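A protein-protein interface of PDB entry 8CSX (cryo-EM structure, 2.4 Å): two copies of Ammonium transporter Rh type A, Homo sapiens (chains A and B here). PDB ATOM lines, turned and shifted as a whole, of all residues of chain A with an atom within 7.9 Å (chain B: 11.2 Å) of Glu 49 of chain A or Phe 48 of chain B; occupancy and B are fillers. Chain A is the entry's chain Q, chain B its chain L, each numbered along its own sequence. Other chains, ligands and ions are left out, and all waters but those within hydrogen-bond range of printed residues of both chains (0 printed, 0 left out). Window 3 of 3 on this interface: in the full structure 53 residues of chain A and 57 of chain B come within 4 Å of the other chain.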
ATOM      1  N   ILE A  46      17.288  29.841  13.320  1.00  0.00           N
ATOM      2  CA  ILE A  46      17.943  29.286  14.497  1.00  0.00           C
ATOM      3  C   ILE A  46      18.356  27.839  14.273  1.00  0.00           C
ATOM      4  O   ILE A  46      19.307  27.368  14.890  1.00  0.00           O
ATOM      5  CB  ILE A  46      17.037  29.385  15.736  1.00  0.00           C
ATOM      6  N   PHE A  47      17.630  27.141  13.393  1.00  0.00           N
ATOM      7  CA  PHE A  47      17.855  25.712  13.200  1.00  0.00           C
ATOM      8  C   PHE A  47      19.278  25.426  12.742  1.00  0.00           C
ATOM      9  O   PHE A  47      19.988  24.617  13.349  1.00  0.00           O
ATOM     10  CB  PHE A  47      16.859  25.158  12.185  1.00  0.00           C
ATOM     11  CG  PHE A  47      17.035  23.697  11.900  1.00  0.00           C
ATOM     12  CD1 PHE A  47      16.415  22.751  12.695  1.00  0.00           C
ATOM     13  CD2 PHE A  47      17.813  23.267  10.836  1.00  0.00           C
ATOM     14  CE1 PHE A  47      16.573  21.405  12.441  1.00  0.00           C
ATOM     15  CE2 PHE A  47      17.973  21.926  10.579  1.00  0.00           C
ATOM     16  CZ  PHE A  47      17.352  20.992  11.386  1.00  0.00           C
ATOM     17  N   PHE A  48      19.713  26.081  11.669  1.00  0.00           N
ATOM     18  CA  PHE A  48      21.041  25.832  11.138  1.00  0.00           C
ATOM     19  C   PHE A  48      22.122  26.598  11.880  1.00  0.00           C
ATOM     20  O   PHE A  48      23.309  26.329  11.666  1.00  0.00           O
ATOM     21  CB  PHE A  48      21.073  26.167   9.649  1.00  0.00           C
ATOM     22  CG  PHE A  48      20.146  25.321   8.830  1.00  0.00           C
ATOM     23  CD1 PHE A  48      20.484  24.021   8.503  1.00  0.00           C
ATOM     24  CD2 PHE A  48      18.925  25.815   8.408  1.00  0.00           C
ATOM     25  CE1 PHE A  48      19.629  23.241   7.760  1.00  0.00           C
ATOM     26  CE2 PHE A  48      18.073  25.037   7.666  1.00  0.00           C
ATOM     27  CZ  PHE A  48      18.426  23.748   7.340  1.00  0.00           C
ATOM     28  N   GLU A  49      21.743  27.539  12.743  1.00  0.00           N
ATOM     29  CA  GLU A  49      22.710  28.123  13.660  1.00  0.00           C
ATOM     30  C   GLU A  49      23.089  27.133  14.752  1.00  0.00           C
ATOM     31  O   GLU A  49      24.259  27.035  15.131  1.00  0.00           O
ATOM     32  CB  GLU A  49      22.146  29.407  14.267  1.00  0.00           C
ATOM     33  N   LEU A  50      22.112  26.378  15.255  1.00  0.00           N
ATOM     34  CA  LEU A  50      22.321  25.474  16.376  1.00  0.00           C
ATOM     35  C   LEU A  50      22.573  24.030  15.965  1.00  0.00           C
ATOM     36  O   LEU A  50      22.933  23.221  16.823  1.00  0.00           O
ATOM     37  CB  LEU A  50      21.114  25.520  17.320  1.00  0.00           C
ATOM     38  CG  LEU A  50      20.862  26.820  18.071  1.00  0.00           C
ATOM     39  CD1 LEU A  50      19.635  26.678  18.956  1.00  0.00           C
ATOM     40  CD2 LEU A  50      22.080  27.210  18.884  1.00  0.00           C
ATOM     41  N   TYR A  51      22.396  23.690  14.688  1.00  0.00           N
ATOM     42  CA  TYR A  51      22.599  22.310  14.253  1.00  0.00           C
ATOM     43  C   TYR A  51      24.008  21.760  14.488  1.00  0.00           C
ATOM     44  O   TYR A  51      24.114  20.576  14.852  1.00  0.00           O
ATOM     45  CB  TYR A  51      22.195  22.167  12.779  1.00  0.00           C
ATOM     46  CG  TYR A  51      22.062  20.726  12.374  1.00  0.00           C
ATOM     47  CD1 TYR A  51      21.070  19.928  12.919  1.00  0.00           C
ATOM     48  CD2 TYR A  51      22.938  20.154  11.467  1.00  0.00           C
ATOM     49  CE1 TYR A  51      20.952  18.612  12.574  1.00  0.00           C
ATOM     50  CE2 TYR A  51      22.824  18.836  11.113  1.00  0.00           C
ATOM     51  CZ  TYR A  51      21.831  18.069  11.668  1.00  0.00           C
ATOM     52  OH  TYR A  51      21.711  16.748  11.316  1.00  0.00           O
ATOM     53  N   PRO A  52      25.106  22.503  14.274  1.00  0.00           N
ATOM     54  CA  PRO A  52      26.422  21.950  14.661  1.00  0.00           C
ATOM     55  C   PRO A  52      26.520  21.571  16.132  1.00  0.00           C
ATOM     56  O   PRO A  52      27.108  20.533  16.478  1.00  0.00           O
ATOM     57  CB  PRO A  52      27.391  23.088  14.311  1.00  0.00           C
ATOM     58  CG  PRO A  52      26.701  23.864  13.272  1.00  0.00           C
ATOM     59  CD  PRO A  52      25.248  23.783  13.553  1.00  0.00           C
ATOM     60  N   LEU A  53      25.940  22.392  17.008  1.00  0.00           N
ATOM     61  CA  LEU A  53      25.952  22.097  18.435  1.00  0.00           C
ATOM     62  C   LEU A  53      25.136  20.851  18.741  1.00  0.00           C
ATOM     63  O   LEU A  53      25.538  20.017  19.564  1.00  0.00           O
ATOM     64  CB  LEU A  53      25.428  23.302  19.219  1.00  0.00           C
ATOM     65  CG  LEU A  53      26.425  24.377  19.657  1.00  0.00           C
ATOM     66  CD1 LEU A  53      27.237  24.926  18.498  1.00  0.00           C
ATOM     67  CD2 LEU A  53      25.685  25.498  20.356  1.00  0.00           C
ATOM     68  N   PHE A  54      23.996  20.694  18.065  1.00  0.00           N
ATOM     69  CA  PHE A  54      23.217  19.476  18.218  1.00  0.00           C
ATOM     70  C   PHE A  54      23.999  18.257  17.752  1.00  0.00           C
ATOM     71  O   PHE A  54      23.882  17.183  18.341  1.00  0.00           O
ATOM     72  CB  PHE A  54      21.901  19.564  17.452  1.00  0.00           C
ATOM     73  CG  PHE A  54      21.208  18.241  17.331  1.00  0.00           C
ATOM     74  CD1 PHE A  54      20.525  17.705  18.411  1.00  0.00           C
ATOM     75  CD2 PHE A  54      21.274  17.509  16.159  1.00  0.00           C
ATOM     76  CE1 PHE A  54      19.906  16.484  18.318  1.00  0.00           C
ATOM     77  CE2 PHE A  54      20.660  16.282  16.065  1.00  0.00           C
ATOM     78  CZ  PHE A  54      19.973  15.771  17.146  1.00  0.00           C
ATOM     79  N   ILE A 112      15.040  22.554  16.418  1.00  0.00           N
ATOM     80  CA  ILE A 112      16.315  21.995  16.842  1.00  0.00           C
ATOM     81  C   ILE A 112      16.390  21.888  18.365  1.00  0.00           C
ATOM     82  O   ILE A 112      17.041  20.980  18.899  1.00  0.00           O
ATOM     83  CB  ILE A 112      17.470  22.821  16.245  1.00  0.00           C
ATOM     84  CG1 ILE A 112      18.803  22.096  16.420  1.00  0.00           C
ATOM     85  CG2 ILE A 112      17.520  24.215  16.845  1.00  0.00           C
ATOM     86  CD1 ILE A 112      18.880  20.796  15.690  1.00  0.00           C
ATOM     87  N   PRO A 223      31.681  21.587  25.584  1.00  0.00           N
ATOM     88  CA  PRO A 223      31.240  22.989  25.416  1.00  0.00           C
ATOM     89  C   PRO A 223      29.953  23.147  24.619  1.00  0.00           C
ATOM     90  O   PRO A 223      29.115  23.994  24.959  1.00  0.00           O
ATOM     91  CB  PRO A 223      32.436  23.637  24.711  1.00  0.00           C
ATOM     92  CG  PRO A 223      33.592  22.868  25.185  1.00  0.00           C
ATOM     93  CD  PRO A 223      33.127  21.454  25.324  1.00  0.00           C
ATOM     94  N   SER A 224      29.759  22.340  23.576  1.00  0.00           N
ATOM     95  CA  SER A 224      28.484  22.353  22.869  1.00  0.00           C
ATOM     96  C   SER A 224      27.359  21.866  23.768  1.00  0.00           C
ATOM     97  O   SER A 224      26.245  22.395  23.717  1.00  0.00           O
ATOM     98  CB  SER A 224      28.564  21.492  21.611  1.00  0.00           C
ATOM     99  OG  SER A 224      29.540  21.976  20.714  1.00  0.00           O
ATOM    100  N   SER A 227      26.463  24.714  26.090  1.00  0.00           N
ATOM    101  CA  SER A 227      26.080  25.985  25.487  1.00  0.00           C
ATOM    102  C   SER A 227      24.941  25.890  24.481  1.00  0.00           C
ATOM    103  O   SER A 227      24.550  26.922  23.931  1.00  0.00           O
ATOM    104  CB  SER A 227      27.285  26.622  24.797  1.00  0.00           C
ATOM    105  OG  SER A 227      27.530  26.003  23.551  1.00  0.00           O
ATOM    106  N   ALA A 228      24.400  24.698  24.227  1.00  0.00           N
ATOM    107  CA  ALA A 228      23.446  24.528  23.131  1.00  0.00           C
ATOM    108  C   ALA A 228      22.152  25.299  23.372  1.00  0.00           C
ATOM    109  O   ALA A 228      21.583  25.878  22.441  1.00  0.00           O
ATOM    110  CB  ALA A 228      23.153  23.045  22.923  1.00  0.00           C
ATOM    111  N   ALA A 230      21.868  27.782  25.660  1.00  0.00           N
ATOM    112  CA  ALA A 230      22.171  29.116  26.152  1.00  0.00           C
ATOM    113  C   ALA A 230      21.728  30.182  25.157  1.00  0.00           C
ATOM    114  O   ALA A 230      21.597  29.930  23.958  1.00  0.00           O
ATOM    115  CB  ALA A 230      23.666  29.251  26.434  1.00  0.00           C
ATOM    116  N   PRO A 232      21.808  33.020  22.584  1.00  0.00           N
ATOM    117  CA  PRO A 232      22.834  33.419  21.613  1.00  0.00           C
ATOM    118  C   PRO A 232      23.410  34.789  21.929  1.00  0.00           C
ATOM    119  O   PRO A 232      22.688  35.719  22.300  1.00  0.00           O
ATOM    120  CB  PRO A 232      22.075  33.425  20.284  1.00  0.00           C
ATOM    121  CG  PRO A 232      20.935  32.497  20.503  1.00  0.00           C
ATOM    122  CD  PRO A 232      20.542  32.658  21.929  1.00  0.00           C
ATOM    123  N   GLY A 233      24.729  34.906  21.771  1.00  0.00           N
ATOM    124  CA  GLY A 233      25.452  36.114  22.103  1.00  0.00           C
ATOM    125  C   GLY A 233      26.435  35.875  23.239  1.00  0.00           C
ATOM    126  O   GLY A 233      27.258  34.953  23.182  1.00  0.00           O
ATOM    127  N   GLN A 236      25.989  32.300  25.365  1.00  0.00           N
ATOM    128  CA  GLN A 236      26.462  31.110  24.667  1.00  0.00           C
ATOM    129  C   GLN A 236      27.985  31.071  24.603  1.00  0.00           C
ATOM    130  O   GLN A 236      28.604  30.028  24.863  1.00  0.00           O
ATOM    131  CB  GLN A 236      25.853  31.067  23.267  1.00  0.00           C
ATOM    132  CG  GLN A 236      26.023  29.748  22.548  1.00  0.00           C
ATOM    133  CD  GLN A 236      24.887  29.465  21.597  1.00  0.00           C
ATOM    134  OE1 GLN A 236      24.725  30.144  20.587  1.00  0.00           O
ATOM    135  NE2 GLN A 236      24.091  28.456  21.913  1.00  0.00           N
ATOM    136  N   CYS A 237      28.606  32.209  24.285  1.00  0.00           N
ATOM    137  CA  CYS A 237      30.060  32.285  24.229  1.00  0.00           C
ATOM    138  C   CYS A 237      30.683  32.063  25.602  1.00  0.00           C
ATOM    139  O   CYS A 237      31.695  31.364  25.718  1.00  0.00           O
ATOM    140  CB  CYS A 237      30.492  33.634  23.645  1.00  0.00           C
ATOM    141  SG  CYS A 237      32.253  34.017  23.805  1.00  0.00           S
ATOM    142  N   ILE A 240      30.593  28.327  26.373  1.00  0.00           N
ATOM    143  CA  ILE A 240      31.635  27.589  25.660  1.00  0.00           C
ATOM    144  C   ILE A 240      32.999  27.812  26.312  1.00  0.00           C
ATOM    145  O   ILE A 240      33.744  26.857  26.575  1.00  0.00           O
ATOM    146  CB  ILE A 240      31.636  27.973  24.169  1.00  0.00           C
ATOM    147  CG1 ILE A 240      30.530  27.218  23.440  1.00  0.00           C
ATOM    148  CG2 ILE A 240      32.979  27.678  23.523  1.00  0.00           C
ATOM    149  CD1 ILE A 240      30.199  27.756  22.082  1.00  0.00           C
ATOM    150  N   PHE B  48      31.021  32.924  16.631  1.00  0.00           N
ATOM    151  CA  PHE B  48      30.238  31.700  16.649  1.00  0.00           C
ATOM    152  C   PHE B  48      30.167  31.107  15.248  1.00  0.00           C
ATOM    153  O   PHE B  48      29.632  30.024  15.049  1.00  0.00           O
ATOM    154  CB  PHE B  48      28.836  31.965  17.198  1.00  0.00           C
ATOM    155  CG  PHE B  48      28.149  30.742  17.713  1.00  0.00           C
ATOM    156  CD1 PHE B  48      28.631  30.085  18.831  1.00  0.00           C
ATOM    157  CD2 PHE B  48      27.016  30.248  17.086  1.00  0.00           C
ATOM    158  CE1 PHE B  48      28.006  28.960  19.312  1.00  0.00           C
ATOM    159  CE2 PHE B  48      26.378  29.119  17.564  1.00  0.00           C
ATOM    160  CZ  PHE B  48      26.872  28.476  18.678  1.00  0.00           C
ATOM    161  N   GLU B  49      30.705  31.851  14.281  1.00  0.00           N
ATOM    162  CA  GLU B  49      30.868  31.342  12.926  1.00  0.00           C
ATOM    163  C   GLU B  49      32.048  30.390  12.816  1.00  0.00           C
ATOM    164  O   GLU B  49      32.016  29.467  12.000  1.00  0.00           O
ATOM    165  CB  GLU B  49      31.049  32.505  11.949  1.00  0.00           C
ATOM    166  N   LEU B  50      33.092  30.603  13.615  1.00  0.00           N
ATOM    167  CA  LEU B  50      34.284  29.772  13.573  1.00  0.00           C
ATOM    168  C   LEU B  50      34.288  28.654  14.606  1.00  0.00           C
ATOM    169  O   LEU B  50      35.262  27.897  14.659  1.00  0.00           O
ATOM    170  CB  LEU B  50      35.531  30.639  13.758  1.00  0.00           C
ATOM    171  CG  LEU B  50      35.799  31.668  12.663  1.00  0.00           C
ATOM    172  CD1 LEU B  50      37.164  32.302  12.853  1.00  0.00           C
ATOM    173  CD2 LEU B  50      35.663  31.053  11.272  1.00  0.00           C
ATOM    174  N   TYR B  51      33.243  28.532  15.422  1.00  0.00           N
ATOM    175  CA  TYR B  51      33.204  27.464  16.418  1.00  0.00           C
ATOM    176  C   TYR B  51      33.236  26.051  15.829  1.00  0.00           C
ATOM    177  O   TYR B  51      33.952  25.204  16.392  1.00  0.00           O
ATOM    178  CB  TYR B  51      31.987  27.651  17.337  1.00  0.00           C
ATOM    179  CG  TYR B  51      31.877  26.588  18.403  1.00  0.00           C
ATOM    180  CD1 TYR B  51      32.822  26.496  19.415  1.00  0.00           C
ATOM    181  CD2 TYR B  51      30.843  25.663  18.387  1.00  0.00           C
ATOM    182  CE1 TYR B  51      32.736  25.518  20.379  1.00  0.00           C
ATOM    183  CE2 TYR B  51      30.751  24.682  19.348  1.00  0.00           C
ATOM    184  CZ  TYR B  51      31.698  24.616  20.343  1.00  0.00           C
ATOM    185  OH  TYR B  51      31.609  23.646  21.305  1.00  0.00           O
ATOM    186  N   PRO B  52      32.500  25.713  14.758  1.00  0.00           N
ATOM    187  CA  PRO B  52      32.659  24.362  14.179  1.00  0.00           C
ATOM    188  C   PRO B  52      34.070  24.040  13.706  1.00  0.00           C
ATOM    189  O   PRO B  52      34.540  22.907  13.888  1.00  0.00           O
ATOM    190  CB  PRO B  52      31.665  24.374  13.013  1.00  0.00           C
ATOM    191  CG  PRO B  52      30.660  25.374  13.393  1.00  0.00           C
ATOM    192  CD  PRO B  52      31.401  26.445  14.099  1.00  0.00           C
ATOM    193  N   LEU B  53      34.763  25.009  13.103  1.00  0.00           N
ATOM    194  CA  LEU B  53      36.155  24.792  12.720  1.00  0.00           C
ATOM    195  C   LEU B  53      37.024  24.561  13.946  1.00  0.00           C
ATOM    196  O   LEU B  53      37.929  23.712  13.929  1.00  0.00           O
ATOM    197  CB  LEU B  53      36.674  25.979  11.914  1.00  0.00           C
ATOM    198  CG  LEU B  53      35.938  26.276  10.609  1.00  0.00           C
ATOM    199  CD1 LEU B  53      36.601  27.424   9.864  1.00  0.00           C
ATOM    200  CD2 LEU B  53      35.867  25.029   9.753  1.00  0.00           C
ATOM    201  N   PHE B  54      36.758  25.309  15.020  1.00  0.00           N
ATOM    202  CA  PHE B  54      37.443  25.061  16.280  1.00  0.00           C
ATOM    203  C   PHE B  54      37.234  23.631  16.746  1.00  0.00           C
ATOM    204  O   PHE B  54      38.165  22.994  17.243  1.00  0.00           O
ATOM    205  CB  PHE B  54      36.958  26.017  17.369  1.00  0.00           C
ATOM    206  CG  PHE B  54      37.160  25.472  18.748  1.00  0.00           C
ATOM    207  CD1 PHE B  54      38.413  25.497  19.331  1.00  0.00           C
ATOM    208  CD2 PHE B  54      36.115  24.875  19.442  1.00  0.00           C
ATOM    209  CE1 PHE B  54      38.617  24.962  20.578  1.00  0.00           C
ATOM    210  CE2 PHE B  54      36.322  24.334  20.691  1.00  0.00           C
ATOM    211  CZ  PHE B  54      37.571  24.381  21.258  1.00  0.00           C
ATOM    212  N   GLN B  55      36.006  23.124  16.636  1.00  0.00           N
ATOM    213  CA  GLN B  55      35.735  21.775  17.117  1.00  0.00           C
ATOM    214  C   GLN B  55      36.450  20.732  16.266  1.00  0.00           C
ATOM    215  O   GLN B  55      36.908  19.706  16.781  1.00  0.00           O
ATOM    216  CB  GLN B  55      34.230  21.516  17.161  1.00  0.00           C
ATOM    217  CG  GLN B  55      33.571  21.950  18.470  1.00  0.00           C
ATOM    218  CD  GLN B  55      34.129  21.220  19.691  1.00  0.00           C
ATOM    219  OE1 GLN B  55      34.665  20.121  19.579  1.00  0.00           O
ATOM    220  NE2 GLN B  55      33.998  21.832  20.862  1.00  0.00           N
ATOM    221  N   ILE B 110      39.039  36.552  25.456  1.00  0.00           N
ATOM    222  CA  ILE B 110      39.098  35.202  24.912  1.00  0.00           C
ATOM    223  C   ILE B 110      37.982  35.039  23.898  1.00  0.00           C
ATOM    224  O   ILE B 110      36.797  35.037  24.255  1.00  0.00           O
ATOM    225  CB  ILE B 110      39.003  34.132  26.012  1.00  0.00           C
ATOM    226  CG1 ILE B 110      40.284  34.117  26.832  1.00  0.00           C
ATOM    227  CG2 ILE B 110      38.764  32.757  25.407  1.00  0.00           C
ATOM    228  CD1 ILE B 110      41.527  34.073  25.993  1.00  0.00           C
ATOM    229  N   GLY B 111      38.362  34.896  22.638  1.00  0.00           N
ATOM    230  CA  GLY B 111      37.409  34.605  21.593  1.00  0.00           C
ATOM    231  C   GLY B 111      37.590  33.200  21.070  1.00  0.00           C
ATOM    232  O   GLY B 111      38.299  32.394  21.676  1.00  0.00           O
ATOM    233  N   ILE B 112      36.949  32.894  19.944  1.00  0.00           N
ATOM    234  CA  ILE B 112      37.129  31.583  19.333  1.00  0.00           C
ATOM    235  C   ILE B 112      38.547  31.444  18.788  1.00  0.00           C
ATOM    236  O   ILE B 112      39.119  30.347  18.773  1.00  0.00           O
ATOM    237  CB  ILE B 112      36.056  31.354  18.249  1.00  0.00           C
ATOM    238  CG1 ILE B 112      36.022  29.892  17.818  1.00  0.00           C
ATOM    239  CG2 ILE B 112      36.257  32.287  17.060  1.00  0.00           C
ATOM    240  CD1 ILE B 112      35.591  28.962  18.914  1.00  0.00           C
ATOM    241  N   LYS B 113      39.147  32.559  18.361  1.00  0.00           N
ATOM    242  CA  LYS B 113      40.474  32.504  17.762  1.00  0.00           C
ATOM    243  C   LYS B 113      41.543  32.228  18.808  1.00  0.00           C
ATOM    244  O   LYS B 113      42.536  31.550  18.525  1.00  0.00           O
ATOM    245  CB  LYS B 113      40.766  33.798  17.008  1.00  0.00           C
ATOM    246  CG  LYS B 113      40.063  33.881  15.673  1.00  0.00           C
ATOM    247  CD  LYS B 113      40.455  35.124  14.911  1.00  0.00           C
ATOM    248  CE  LYS B 113      39.788  35.156  13.545  1.00  0.00           C
ATOM    249  NZ  LYS B 113      40.170  36.366  12.770  1.00  0.00           N
ATOM    250  N   ASN B 114      41.350  32.732  20.028  1.00  0.00           N
ATOM    251  CA  ASN B 114      42.252  32.387  21.121  1.00  0.00           C
ATOM    252  C   ASN B 114      42.227  30.890  21.399  1.00  0.00           C
ATOM    253  O   ASN B 114      43.275  30.272  21.604  1.00  0.00           O
ATOM    254  CB  ASN B 114      41.878  33.166  22.380  1.00  0.00           C
ATOM    255  CG  ASN B 114      41.959  34.656  22.184  1.00  0.00           C
ATOM    256  OD1 ASN B 114      40.967  35.301  21.867  1.00  0.00           O
ATOM    257  ND2 ASN B 114      43.150  35.214  22.362  1.00  0.00           N
ATOM    258  N   MET B 115      41.036  30.292  21.402  1.00  0.00           N
ATOM    259  CA  MET B 115      40.926  28.858  21.638  1.00  0.00           C
ATOM    260  C   MET B 115      41.563  28.062  20.507  1.00  0.00           C
ATOM    261  O   MET B 115      42.248  27.060  20.751  1.00  0.00           O
ATOM    262  CB  MET B 115      39.461  28.473  21.820  1.00  0.00           C
ATOM    263  CG  MET B 115      38.784  29.156  23.002  1.00  0.00           C
ATOM    264  SD  MET B 115      36.984  29.124  22.907  1.00  0.00           S
ATOM    265  CE  MET B 115      36.651  27.371  22.865  1.00  0.00           C
ATOM    266  N   ILE B 116      41.352  28.494  19.262  1.00  0.00           N
ATOM    267  CA  ILE B 116      41.951  27.804  18.123  1.00  0.00           C
ATOM    268  C   ILE B 116      43.473  27.872  18.196  1.00  0.00           C
ATOM    269  O   ILE B 116      44.167  26.871  17.970  1.00  0.00           O
ATOM    270  CB  ILE B 116      41.398  28.383  16.806  1.00  0.00           C
ATOM    271  CG1 ILE B 116      39.922  28.018  16.659  1.00  0.00           C
ATOM    272  CG2 ILE B 116      42.179  27.863  15.615  1.00  0.00           C
ATOM    273  CD1 ILE B 116      39.161  28.866  15.685  1.00  0.00           C
ATOM    274  N   ALA B 228      41.080  27.506   9.557  1.00  0.00           N
ATOM    275  CA  ALA B 228      40.297  28.057  10.658  1.00  0.00           C
ATOM    276  C   ALA B 228      40.586  29.540  10.868  1.00  0.00           C
ATOM    277  O   ALA B 228      39.664  30.342  11.039  1.00  0.00           O
ATOM    278  CB  ALA B 228      40.570  27.265  11.936  1.00  0.00           C
ATOM    279  N   GLN B 236      39.910  31.592   2.851  1.00  0.00           N
ATOM    280  CA  GLN B 236      39.460  30.435   3.617  1.00  0.00           C
ATOM    281  C   GLN B 236      38.963  29.321   2.700  1.00  0.00           C
ATOM    282  O   GLN B 236      39.253  28.138   2.928  1.00  0.00           O
ATOM    283  CB  GLN B 236      38.376  30.860   4.609  1.00  0.00           C
ATOM    284  CG  GLN B 236      37.961  29.783   5.583  1.00  0.00           C
ATOM    285  CD  GLN B 236      37.357  30.344   6.855  1.00  0.00           C
ATOM    286  OE1 GLN B 236      36.272  30.917   6.840  1.00  0.00           O
ATOM    287  NE2 GLN B 236      38.068  30.187   7.965  1.00  0.00           N
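The side-chain hydroxyl of Tyr 51 of chain B is in hydrogen-bond range of the side-chain hydroxyl of Ser 224 of chain A, at 2.7 Å.
The side-chain hydroxyl (OH) of Tyr 51 of chain B is in hydrogen-bond range of the side-chain amide nitrogen (NE2) of Gln 55 of chain B (3.0 Å). The backbone carbonyl oxygen (O) of Ser 227 of chain A sits at hydrogen-bond distance from the side-chain amide nitrogen (NE2) of Gln 236 of chain A (2.6 Å). O of Pro 223 of chain A is in hydrogen-bond range of OG of Ser 227 of chain A (2.9 Å).
Phe 48 of chain B touches Glu 49 of chain A. Phe 48 of chain B touches Leu 53 of chain A (CZ to CD1, 3.6 Å). Leu 53 of chain A touches Tyr 51 of chain B (CD1 to CE2, 3.6 Å). Pro 223 of chain A touches Tyr 51 of chain B. Phe 48 of chain B touches Gln 236 of chain A. Phe 48 of chain B touches Ile 240 of chain A (CE1 to CD1, 3.7 Å). Ile 240 of chain A touches Tyr 51 of chain B (CD1 to CE1, 3.8 Å). Met 115 of chain B touches Ile 240 of chain A (CE to CG2, 3.7 Å).
No residue of chain B comes within 4 Å of Ile 46 of chain A. No residue of chain B comes within 4 Å of Leu 50 of chain A. Of the printed residues of chain A, Met 115 of chain B touches Ile 240 (3.7 Å). Printed residues of chain B within 4 Å of Pro 223 of chain A: Tyr 51 (3.5 Å). Of the printed residues of chain B, Leu 53 of chain A touches Phe 48 (3.6 Å) and Tyr 51 (3.6 Å). Printed residues of chain A within 4 Å of Tyr 51 of chain B: Leu 53 (3.6 Å), Pro 223 (3.5 Å), Ser 224 (2.7 Å) and Ile 240 (3.8 Å). Ser 227 of chain A touches none of the printed residues of chain B. Gly 111 of chain B touches none of the printed residues of chain A. The nearest printed residue of chain B that does not touch Ile 240 of chain A is Ile 112 of chain B (5.5 Å).
Hydrophobic or aromatic side chains of chain B that line the printed part of chain A: Phe 48, Tyr 51 and Met 115. Of the 20 printed residues of chain A, 6 touch a printed residue of chain B. Printed residues of chain A that touch a printed residue of chain B: Glu 49, Leu 53, Pro 223, Ser 224, Gln 236 and Ile 240. Among the printed residues, 9 pairs touch across the chains. Among the printed residues, no Asp or Glu carboxylate lies within 4 Å of a Lys or Arg side-chain nitrogen of the other chain.
Glu 49 of chain A touches Phe 48 of chain B, but with the chains exchanged Phe 48 of chain A does not touch Glu 49 of chain B (9.2 Å). Leu 53 of chain A touches Phe 48 of chain B, but with the chains exchanged Phe 48 of chain A does not touch Leu 53 of chain B (11.6 Å). Leu 53 of chain A touches Tyr 51 of chain B, but with the chains exchanged Tyr 51 of chain A does not touch Leu 53 of chain B (11.3 Å). Gln 236 of chain A touches Phe 48 of chain B, but with the chains exchanged Phe 48 of chain A does not touch Gln 236 of chain B (14.6 Å). 10 positions are printed for both chains.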
